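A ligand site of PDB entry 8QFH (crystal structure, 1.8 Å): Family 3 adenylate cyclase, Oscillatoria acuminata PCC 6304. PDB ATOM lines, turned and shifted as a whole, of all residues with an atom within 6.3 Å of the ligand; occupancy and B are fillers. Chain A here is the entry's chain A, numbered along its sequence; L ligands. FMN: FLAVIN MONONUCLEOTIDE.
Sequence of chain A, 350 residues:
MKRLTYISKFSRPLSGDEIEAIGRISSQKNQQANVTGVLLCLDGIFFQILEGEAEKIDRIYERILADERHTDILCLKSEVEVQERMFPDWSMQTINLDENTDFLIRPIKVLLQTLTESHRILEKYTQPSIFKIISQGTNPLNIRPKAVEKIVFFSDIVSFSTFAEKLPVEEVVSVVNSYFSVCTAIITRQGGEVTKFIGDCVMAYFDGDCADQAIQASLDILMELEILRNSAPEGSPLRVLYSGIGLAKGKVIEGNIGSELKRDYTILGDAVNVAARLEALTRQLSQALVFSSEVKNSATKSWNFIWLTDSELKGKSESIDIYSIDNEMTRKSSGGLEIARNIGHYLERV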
ATOM      1  N   TYR A   6      -2.016 -12.019  -6.816  1.00  0.00           N
ATOM      2  CA  TYR A   6      -3.378 -12.493  -6.957  1.00  0.00           C
ATOM      3  C   TYR A   6      -3.817 -12.405  -8.424  1.00  0.00           C
ATOM      4  O   TYR A   6      -3.181 -11.755  -9.257  1.00  0.00           O
ATOM      5  CB  TYR A   6      -4.361 -11.715  -6.059  1.00  0.00           C
ATOM      6  CG  TYR A   6      -4.702 -10.320  -6.542  1.00  0.00           C
ATOM      7  CD1 TYR A   6      -5.706 -10.118  -7.466  1.00  0.00           C
ATOM      8  CD2 TYR A   6      -4.000  -9.213  -6.068  1.00  0.00           C
ATOM      9  CE1 TYR A   6      -6.003  -8.847  -7.935  1.00  0.00           C
ATOM     10  CE2 TYR A   6      -4.296  -7.934  -6.524  1.00  0.00           C
ATOM     11  CZ  TYR A   6      -5.309  -7.760  -7.454  1.00  0.00           C
ATOM     12  OH  TYR A   6      -5.595  -6.497  -7.919  1.00  0.00           O
ATOM     13  N   SER A   8      -7.676 -12.095 -10.724  1.00  0.00           N
ATOM     14  CA  SER A   8      -9.100 -11.778 -10.617  1.00  0.00           C
ATOM     15  C   SER A   8      -9.702 -11.741 -12.002  1.00  0.00           C
ATOM     16  O   SER A   8      -8.996 -11.750 -13.011  1.00  0.00           O
ATOM     17  CB  SER A   8      -9.322 -10.448  -9.882  1.00  0.00           C
ATOM     18  OG  SER A   8      -8.822  -9.371 -10.658  1.00  0.00           O
ATOM     19  N   LEU A  14     -13.973  -3.940 -19.756  1.00  0.00           N
ATOM     20  CA  LEU A  14     -13.196  -2.734 -19.499  1.00  0.00           C
ATOM     21  C   LEU A  14     -12.429  -2.375 -20.764  1.00  0.00           C
ATOM     22  O   LEU A  14     -11.786  -3.246 -21.366  1.00  0.00           O
ATOM     23  CB  LEU A  14     -12.225  -2.937 -18.328  1.00  0.00           C
ATOM     24  CG  LEU A  14     -12.796  -3.451 -17.012  1.00  0.00           C
ATOM     25  CD1 LEU A  14     -11.672  -3.620 -15.994  1.00  0.00           C
ATOM     26  CD2 LEU A  14     -13.861  -2.508 -16.485  1.00  0.00           C
ATOM     27  N   ILE A  22      -6.752   2.933 -14.282  1.00  0.00           N
ATOM     28  CA  ILE A  22      -6.490   2.188 -13.050  1.00  0.00           C
ATOM     29  C   ILE A  22      -4.996   2.208 -12.733  1.00  0.00           C
ATOM     30  O   ILE A  22      -4.593   2.414 -11.585  1.00  0.00           O
ATOM     31  CB  ILE A  22      -7.025   0.752 -13.163  1.00  0.00           C
ATOM     32  CG1 ILE A  22      -8.561   0.753 -13.117  1.00  0.00           C
ATOM     33  CG2 ILE A  22      -6.438  -0.127 -12.038  1.00  0.00           C
ATOM     34  CD1 ILE A  22      -9.184  -0.527 -13.636  1.00  0.00           C
ATOM     35  N   ILE A  25      -3.904   5.871 -11.482  1.00  0.00           N
ATOM     36  CA  ILE A  25      -4.253   6.155 -10.095  1.00  0.00           C
ATOM     37  C   ILE A  25      -3.456   5.260  -9.160  1.00  0.00           C
ATOM     38  O   ILE A  25      -3.002   5.696  -8.098  1.00  0.00           O
ATOM     39  CB  ILE A  25      -5.771   5.997  -9.877  1.00  0.00           C
ATOM     40  CG1 ILE A  25      -6.524   7.166 -10.512  1.00  0.00           C
ATOM     41  CG2 ILE A  25      -6.091   5.901  -8.396  1.00  0.00           C
ATOM     42  CD1 ILE A  25      -7.961   6.847 -10.855  1.00  0.00           C
ATOM     43  N   SER A  26      -3.286   3.994  -9.550  1.00  0.00           N
ATOM     44  CA  SER A  26      -2.507   3.064  -8.735  1.00  0.00           C
ATOM     45  C   SER A  26      -1.069   3.555  -8.567  1.00  0.00           C
ATOM     46  O   SER A  26      -0.496   3.471  -7.481  1.00  0.00           O
ATOM     47  CB  SER A  26      -2.511   1.674  -9.371  1.00  0.00           C
ATOM     48  OG  SER A  26      -3.798   1.103  -9.392  1.00  0.00           O
ATOM     49  N   SER A  27      -0.475   4.040  -9.662  1.00  0.00           N
ATOM     50  CA  SER A  27       0.890   4.566  -9.590  1.00  0.00           C
ATOM     51  C   SER A  27       0.968   5.718  -8.602  1.00  0.00           C
ATOM     52  O   SER A  27       1.891   5.779  -7.779  1.00  0.00           O
ATOM     53  CB  SER A  27       1.330   5.028 -10.977  1.00  0.00           C
ATOM     54  OG  SER A  27       2.689   5.423 -10.954  1.00  0.00           O
ATOM     55  N   LYS A  29      -0.923   6.557  -5.998  1.00  0.00           N
ATOM     56  CA  LYS A  29      -1.108   6.202  -4.601  1.00  0.00           C
ATOM     57  C   LYS A  29       0.048   5.332  -4.101  1.00  0.00           C
ATOM     58  O   LYS A  29       0.557   5.546  -2.995  1.00  0.00           O
ATOM     59  CB  LYS A  29      -2.447   5.493  -4.425  1.00  0.00           C
ATOM     60  CG  LYS A  29      -3.640   6.404  -4.688  1.00  0.00           C
ATOM     61  CD  LYS A  29      -4.979   5.672  -4.635  1.00  0.00           C
ATOM     62  CE  LYS A  29      -5.463   5.507  -3.207  1.00  0.00           C
ATOM     63  NZ  LYS A  29      -5.614   6.815  -2.497  1.00  0.00           N
ATOM     64  N   ASN A  30       0.476   4.365  -4.900  1.00  0.00           N
ATOM     65  CA  ASN A  30       1.539   3.462  -4.464  1.00  0.00           C
ATOM     66  C   ASN A  30       2.836   4.220  -4.209  1.00  0.00           C
ATOM     67  O   ASN A  30       3.542   3.940  -3.230  1.00  0.00           O
ATOM     68  CB  ASN A  30       1.768   2.372  -5.515  1.00  0.00           C
ATOM     69  CG  ASN A  30       0.636   1.353  -5.558  1.00  0.00           C
ATOM     70  OD1 ASN A  30      -0.346   1.450  -4.825  1.00  0.00           O
ATOM     71  ND2 ASN A  30       0.773   0.375  -6.443  1.00  0.00           N
ATOM     72  N   VAL A  35       5.074   1.568  -2.200  1.00  0.00           N
ATOM     73  CA  VAL A  35       4.639   0.274  -2.701  1.00  0.00           C
ATOM     74  C   VAL A  35       5.043   0.179  -4.164  1.00  0.00           C
ATOM     75  O   VAL A  35       5.007   1.190  -4.885  1.00  0.00           O
ATOM     76  CB  VAL A  35       3.121   0.098  -2.523  1.00  0.00           C
ATOM     77  CG1 VAL A  35       2.600  -1.056  -3.351  1.00  0.00           C
ATOM     78  CG2 VAL A  35       2.782  -0.074  -1.039  1.00  0.00           C
ATOM     79  N   LEU A  39       0.892  -4.814 -12.846  1.00  0.00           N
ATOM     80  CA  LEU A  39      -0.492  -5.167 -13.115  1.00  0.00           C
ATOM     81  C   LEU A  39      -0.580  -5.612 -14.565  1.00  0.00           C
ATOM     82  O   LEU A  39      -0.252  -4.849 -15.469  1.00  0.00           O
ATOM     83  CB  LEU A  39      -1.415  -3.964 -12.865  1.00  0.00           C
ATOM     84  CG  LEU A  39      -2.898  -4.137 -13.219  1.00  0.00           C
ATOM     85  CD1 LEU A  39      -3.491  -5.291 -12.427  1.00  0.00           C
ATOM     86  CD2 LEU A  39      -3.673  -2.846 -12.969  1.00  0.00           C
ATOM     87  N   PHE A  46      -7.189 -10.171 -14.609  1.00  0.00           N
ATOM     88  CA  PHE A  46      -6.138  -9.355 -14.021  1.00  0.00           C
ATOM     89  C   PHE A  46      -5.161 -10.257 -13.278  1.00  0.00           C
ATOM     90  O   PHE A  46      -5.565 -11.215 -12.616  1.00  0.00           O
ATOM     91  CB  PHE A  46      -6.695  -8.348 -13.010  1.00  0.00           C
ATOM     92  CG  PHE A  46      -7.347  -7.135 -13.615  1.00  0.00           C
ATOM     93  CD1 PHE A  46      -6.632  -6.247 -14.399  1.00  0.00           C
ATOM     94  CD2 PHE A  46      -8.672  -6.850 -13.341  1.00  0.00           C
ATOM     95  CE1 PHE A  46      -7.228  -5.111 -14.920  1.00  0.00           C
ATOM     96  CE2 PHE A  46      -9.279  -5.713 -13.853  1.00  0.00           C
ATOM     97  CZ  PHE A  46      -8.549  -4.848 -14.649  1.00  0.00           C
ATOM     98  N   GLN A  48      -1.873  -9.374 -10.561  1.00  0.00           N
ATOM     99  CA  GLN A  48      -1.142  -8.286  -9.924  1.00  0.00           C
ATOM    100  C   GLN A  48      -0.175  -8.810  -8.873  1.00  0.00           C
ATOM    101  O   GLN A  48      -0.465  -9.789  -8.167  1.00  0.00           O
ATOM    102  CB  GLN A  48      -2.087  -7.273  -9.277  1.00  0.00           C
ATOM    103  CG  GLN A  48      -1.368  -6.046  -8.696  1.00  0.00           C
ATOM    104  CD  GLN A  48      -2.316  -4.920  -8.356  1.00  0.00           C
ATOM    105  OE1 GLN A  48      -3.352  -5.145  -7.725  1.00  0.00           O
ATOM    106  NE2 GLN A  48      -1.981  -3.703  -8.765  1.00  0.00           N
ATOM    107  N   LEU A  50       2.056  -7.010  -5.691  1.00  0.00           N
ATOM    108  CA  LEU A  50       2.252  -5.809  -4.877  1.00  0.00           C
ATOM    109  C   LEU A  50       3.280  -6.100  -3.786  1.00  0.00           C
ATOM    110  O   LEU A  50       3.226  -7.160  -3.146  1.00  0.00           O
ATOM    111  CB  LEU A  50       0.954  -5.363  -4.208  1.00  0.00           C
ATOM    112  CG  LEU A  50      -0.233  -4.943  -5.073  1.00  0.00           C
ATOM    113  CD1 LEU A  50      -1.515  -5.092  -4.258  1.00  0.00           C
ATOM    114  CD2 LEU A  50      -0.076  -3.518  -5.563  1.00  0.00           C
ATOM    115  N   ILE A  60      -3.928  -1.558   1.225  1.00  0.00           N
ATOM    116  CA  ILE A  60      -4.195  -1.425  -0.209  1.00  0.00           C
ATOM    117  C   ILE A  60      -4.968  -2.629  -0.726  1.00  0.00           C
ATOM    118  O   ILE A  60      -5.919  -2.492  -1.497  1.00  0.00           O
ATOM    119  CB  ILE A  60      -2.873  -1.212  -0.979  1.00  0.00           C
ATOM    120  CG1 ILE A  60      -2.357   0.218  -0.781  1.00  0.00           C
ATOM    121  CG2 ILE A  60      -3.065  -1.466  -2.469  1.00  0.00           C
ATOM    122  CD1 ILE A  60      -0.879   0.301  -0.503  1.00  0.00           C
ATOM    123  N   ARG A  63      -8.653  -2.431  -0.008  1.00  0.00           N
ATOM    124  CA  ARG A  63      -9.333  -1.485  -0.886  1.00  0.00           C
ATOM    125  C   ARG A  63      -9.520  -2.067  -2.287  1.00  0.00           C
ATOM    126  O   ARG A  63     -10.553  -1.843  -2.928  1.00  0.00           O
ATOM    127  CB  ARG A  63      -8.537  -0.180  -0.930  1.00  0.00           C
ATOM    128  CG  ARG A  63      -8.834   0.742  -2.103  1.00  0.00           C
ATOM    129  CD  ARG A  63     -10.268   1.230  -2.108  1.00  0.00           C
ATOM    130  NE  ARG A  63     -11.010   0.670  -3.233  1.00  0.00           N
ATOM    131  CZ  ARG A  63     -12.332   0.603  -3.301  1.00  0.00           C
ATOM    132  NH1 ARG A  63     -13.096   1.042  -2.320  1.00  0.00           N
ATOM    133  NH2 ARG A  63     -12.891   0.081  -4.390  1.00  0.00           N
ATOM    134  N   ILE A  64      -8.531  -2.809  -2.771  1.00  0.00           N
ATOM    135  CA  ILE A  64      -8.661  -3.460  -4.075  1.00  0.00           C
ATOM    136  C   ILE A  64      -9.768  -4.505  -4.045  1.00  0.00           C
ATOM    137  O   ILE A  64     -10.468  -4.710  -5.044  1.00  0.00           O
ATOM    138  CB  ILE A  64      -7.314  -4.071  -4.505  1.00  0.00           C
ATOM    139  CG1 ILE A  64      -6.320  -2.987  -4.920  1.00  0.00           C
ATOM    140  CG2 ILE A  64      -7.519  -5.060  -5.648  1.00  0.00           C
ATOM    141  CD1 ILE A  64      -4.850  -3.453  -4.867  1.00  0.00           C
ATOM    142  N   LEU A  65      -9.954  -5.183  -2.904  1.00  0.00           N
ATOM    143  CA  LEU A  65     -11.015  -6.185  -2.808  1.00  0.00           C
ATOM    144  C   LEU A  65     -12.388  -5.562  -2.948  1.00  0.00           C
ATOM    145  O   LEU A  65     -13.344  -6.257  -3.324  1.00  0.00           O
ATOM    146  CB  LEU A  65     -10.951  -6.934  -1.476  1.00  0.00           C
ATOM    147  CG  LEU A  65      -9.677  -7.738  -1.205  1.00  0.00           C
ATOM    148  CD1 LEU A  65      -9.661  -8.249   0.226  1.00  0.00           C
ATOM    149  CD2 LEU A  65      -9.573  -8.890  -2.182  1.00  0.00           C
ATOM    150  N   ALA A  66     -12.524  -4.283  -2.617  1.00  0.00           N
ATOM    151  CA  ALA A  66     -13.808  -3.606  -2.689  1.00  0.00           C
ATOM    152  C   ALA A  66     -14.101  -3.011  -4.057  1.00  0.00           C
ATOM    153  O   ALA A  66     -15.220  -2.521  -4.266  1.00  0.00           O
ATOM    154  CB  ALA A  66     -13.865  -2.495  -1.632  1.00  0.00           C
ATOM    155  N   ASP A  67     -13.148  -3.042  -4.992  1.00  0.00           N
ATOM    156  CA  ASP A  67     -13.322  -2.431  -6.305  1.00  0.00           C
ATOM    157  C   ASP A  67     -14.343  -3.216  -7.110  1.00  0.00           C
ATOM    158  O   ASP A  67     -14.171  -4.406  -7.352  1.00  0.00           O
ATOM    159  CB  ASP A  67     -11.987  -2.366  -7.047  1.00  0.00           C
ATOM    160  CG  ASP A  67     -11.980  -1.322  -8.159  1.00  0.00           C
ATOM    161  OD1 ASP A  67     -12.814  -1.433  -9.077  1.00  0.00           O
ATOM    162  OD2 ASP A  67     -11.129  -0.409  -8.133  1.00  0.00           O
ATOM    163  N   ARG A  69     -14.888  -3.322 -10.130  1.00  0.00           N
ATOM    164  CA  ARG A  69     -14.513  -3.664 -11.501  1.00  0.00           C
ATOM    165  C   ARG A  69     -13.928  -5.059 -11.647  1.00  0.00           C
ATOM    166  O   ARG A  69     -13.672  -5.482 -12.787  1.00  0.00           O
ATOM    167  CB  ARG A  69     -13.516  -2.639 -12.040  1.00  0.00           C
ATOM    168  CG  ARG A  69     -14.129  -1.253 -12.166  1.00  0.00           C
ATOM    169  CD  ARG A  69     -13.110  -0.201 -12.495  1.00  0.00           C
ATOM    170  NE  ARG A  69     -12.407   0.218 -11.295  1.00  0.00           N
ATOM    171  CZ  ARG A  69     -11.607   1.267 -11.220  1.00  0.00           C
ATOM    172  NH1 ARG A  69     -11.451   2.092 -12.239  1.00  0.00           N
ATOM    173  NH2 ARG A  69     -10.947   1.506 -10.090  1.00  0.00           N
ATOM    174  N   HIS A  70     -13.711  -5.790 -10.562  1.00  0.00           N
ATOM    175  CA  HIS A  70     -13.276  -7.173 -10.706  1.00  0.00           C
ATOM    176  C   HIS A  70     -13.905  -7.995  -9.595  1.00  0.00           C
ATOM    177  O   HIS A  70     -14.510  -7.474  -8.664  1.00  0.00           O
ATOM    178  CB  HIS A  70     -11.739  -7.288 -10.754  1.00  0.00           C
ATOM    179  CG  HIS A  70     -11.018  -6.854  -9.515  1.00  0.00           C
ATOM    180  ND1 HIS A  70      -9.686  -7.127  -9.308  1.00  0.00           N
ATOM    181  CD2 HIS A  70     -11.430  -6.166  -8.420  1.00  0.00           C
ATOM    182  CE1 HIS A  70      -9.296  -6.628  -8.147  1.00  0.00           C
ATOM    183  NE2 HIS A  70     -10.342  -6.040  -7.585  1.00  0.00           N
ATOM    184  N   SER A  91       6.154   1.912  -9.403  1.00  0.00           N
ATOM    185  CA  SER A  91       5.087   2.092  -8.417  1.00  0.00           C
ATOM    186  C   SER A  91       3.881   1.228  -8.756  1.00  0.00           C
ATOM    187  O   SER A  91       3.252   0.645  -7.874  1.00  0.00           O
ATOM    188  CB  SER A  91       4.706   3.566  -8.335  1.00  0.00           C
ATOM    189  OG  SER A  91       5.708   4.300  -7.649  1.00  0.00           O
ATOM    190  N   MET A  92       3.543   1.150 -10.044  1.00  0.00           N
ATOM    191  CA  MET A  92       2.565   0.197 -10.563  1.00  0.00           C
ATOM    192  C   MET A  92       2.679   0.187 -12.073  1.00  0.00           C
ATOM    193  O   MET A  92       2.078   1.035 -12.754  1.00  0.00           O
ATOM    194  CB  MET A  92       1.125   0.523 -10.157  1.00  0.00           C
ATOM    195  CG  MET A  92       0.127  -0.629 -10.402  1.00  0.00           C
ATOM    196  SD  MET A  92       0.760  -2.315 -10.268  1.00  0.00           S
ATOM    197  CE  MET A  92       1.292  -2.272  -8.562  1.00  0.00           C
HETATM  198  N1  FMN L   1      -5.295   1.315  -6.148  1.00  0.00           N
HETATM  199  C2  FMN L   1      -4.009   1.639  -5.506  1.00  0.00           C
HETATM  200  O2  FMN L   1      -3.910   2.603  -4.835  1.00  0.00           O
HETATM  201  N3  FMN L   1      -2.849   0.732  -5.713  1.00  0.00           N
HETATM  202  C4  FMN L   1      -2.981  -0.447  -6.544  1.00  0.00           C
HETATM  203  O4  FMN L   1      -2.032  -1.156  -6.708  1.00  0.00           O
HETATM  204  C4A FMN L   1      -4.313  -0.760  -7.185  1.00  0.00           C
HETATM  205  N5  FMN L   1      -4.495  -1.921  -8.011  1.00  0.00           N
HETATM  206  C5A FMN L   1      -5.816  -2.204  -8.622  1.00  0.00           C
HETATM  207  C6  FMN L   1      -5.946  -3.352  -9.414  1.00  0.00           C
HETATM  208  C7  FMN L   1      -7.179  -3.612  -9.996  1.00  0.00           C
HETATM  209  C7M FMN L   1      -6.994  -4.914 -10.777  1.00  0.00           C
HETATM  210  C8  FMN L   1      -8.263  -2.755  -9.804  1.00  0.00           C
HETATM  211  C8M FMN L   1      -9.561  -3.153 -10.489  1.00  0.00           C
HETATM  212  C9  FMN L   1      -8.128  -1.615  -9.016  1.00  0.00           C
HETATM  213  C9A FMN L   1      -6.898  -1.339  -8.418  1.00  0.00           C
HETATM  214  N10 FMN L   1      -6.714  -0.127  -7.567  1.00  0.00           N
HETATM  215  C10 FMN L   1      -5.433   0.130  -6.974  1.00  0.00           C
HETATM  216  C1' FMN L   1      -7.780   0.829  -7.350  1.00  0.00           C
HETATM  217  C2' FMN L   1      -8.476   0.768  -6.013  1.00  0.00           C
HETATM  218  O2' FMN L   1      -9.343  -0.324  -6.080  1.00  0.00           O
HETATM  219  C3' FMN L   1      -9.248   2.081  -5.847  1.00  0.00           C
HETATM  220  O3' FMN L   1     -10.007   2.362  -6.980  1.00  0.00           O
HETATM  221  C4' FMN L   1      -8.317   3.283  -5.675  1.00  0.00           C
HETATM  222  O4' FMN L   1      -7.253   2.980  -4.806  1.00  0.00           O
HETATM  223  C5' FMN L   1      -9.119   4.435  -5.103  1.00  0.00           C
HETATM  224  O5' FMN L   1      -8.369   5.589  -5.322  1.00  0.00           O
HETATM  225  P   FMN L   1      -9.000   7.014  -4.809  1.00  0.00           P
HETATM  226  O1P FMN L   1      -7.880   8.015  -4.649  1.00  0.00           O
HETATM  227  O2P FMN L   1      -9.997   7.507  -5.834  1.00  0.00           O
HETATM  228  O3P FMN L   1      -9.693   6.760  -3.490  1.00  0.00           O
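Merely in contact with the ligand: Tyr 6 (3.5 Å), Ile 22 (3.8 Å), Ile 25 (3.8 Å), Leu 39 (3.9 Å), Phe 46 (3.6 Å), Leu 50 (3.3 Å), Ile 60 (3.9 Å), Ile 64 (3.5 Å), His 70 (3.8 Å) and Met 92 (3.97 Å). Within 4 Å of the ligand: Tyr 6, Ile 22, Ile 25, Ser 26, Lys 29, Asn 30, Leu 39, Phe 46, Gln 48, Leu 50, Ile 60, Arg 63, Ile 64, Asp 67, Arg 69, His 70 and Met 92. The nearest printed residue that does not touch the ligand is Ser 8 (4.8 Å).
The side-chain hydroxyl (OG) of Ser 8 sits at hydrogen-bond distance from a ring nitrogen (ND1) of His 70. The side-chain amide oxygen (OD1) of Asn 30 sits close to the backbone carbonyl oxygen (O) of Ser 26, at 3.3 Å. The backbone carbonyl oxygen (O) of Asn 30 is in hydrogen-bond range of the backbone NH (N) of Val 35 (3.0 Å). The side-chain hydroxyl (OH) of Tyr 6 lies within hydrogen-bond range of the side-chain amide oxygen (OE1) of Gln 48 (2.6 Å). SD of Met 92 lies within hydrogen-bond range of NE2 of Gln 48 (3.4 Å). The backbone carbonyl oxygen of Ala 66 lies close to the guanidinium group of Arg 63 (3.5 Å). OD2 of Asp 67 lies within salt-bridge range of NH2 of Arg 69 (2.7 Å). The backbone carbonyl oxygen of Ser 91 is in hydrogen-bond range of the side-chain amide nitrogen of Asn 30 (2.9 Å).
The side-chain amino group of Lys 29 lies within salt-bridge range of an oxygen (O1P) of the ligand (3.3 Å). The side-chain amide oxygen (OD1) of Asn 30 sits at hydrogen-bond distance from a nitrogen (N3) of the ligand (2.8 Å). NE2 of Gln 48 is in hydrogen-bond range of N5 of the ligand, 3.2 Å away. An oxygen (O2') of the ligand is in hydrogen-bond range of the guanidinium group (NE) of Arg 63, at 3.4 Å. The side-chain hydroxyl (OG) of Ser 26 lies close to a nitrogen (N5) of the ligand (3.4 Å). The side-chain carboxylate (OD2) of Asp 67 lies within hydrogen-bond range of an oxygen (O2') of the ligand (2.7 Å). The guanidinium group of Arg 69 is in hydrogen-bond range of an oxygen (O3') of the ligand, at 3.4 Å.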
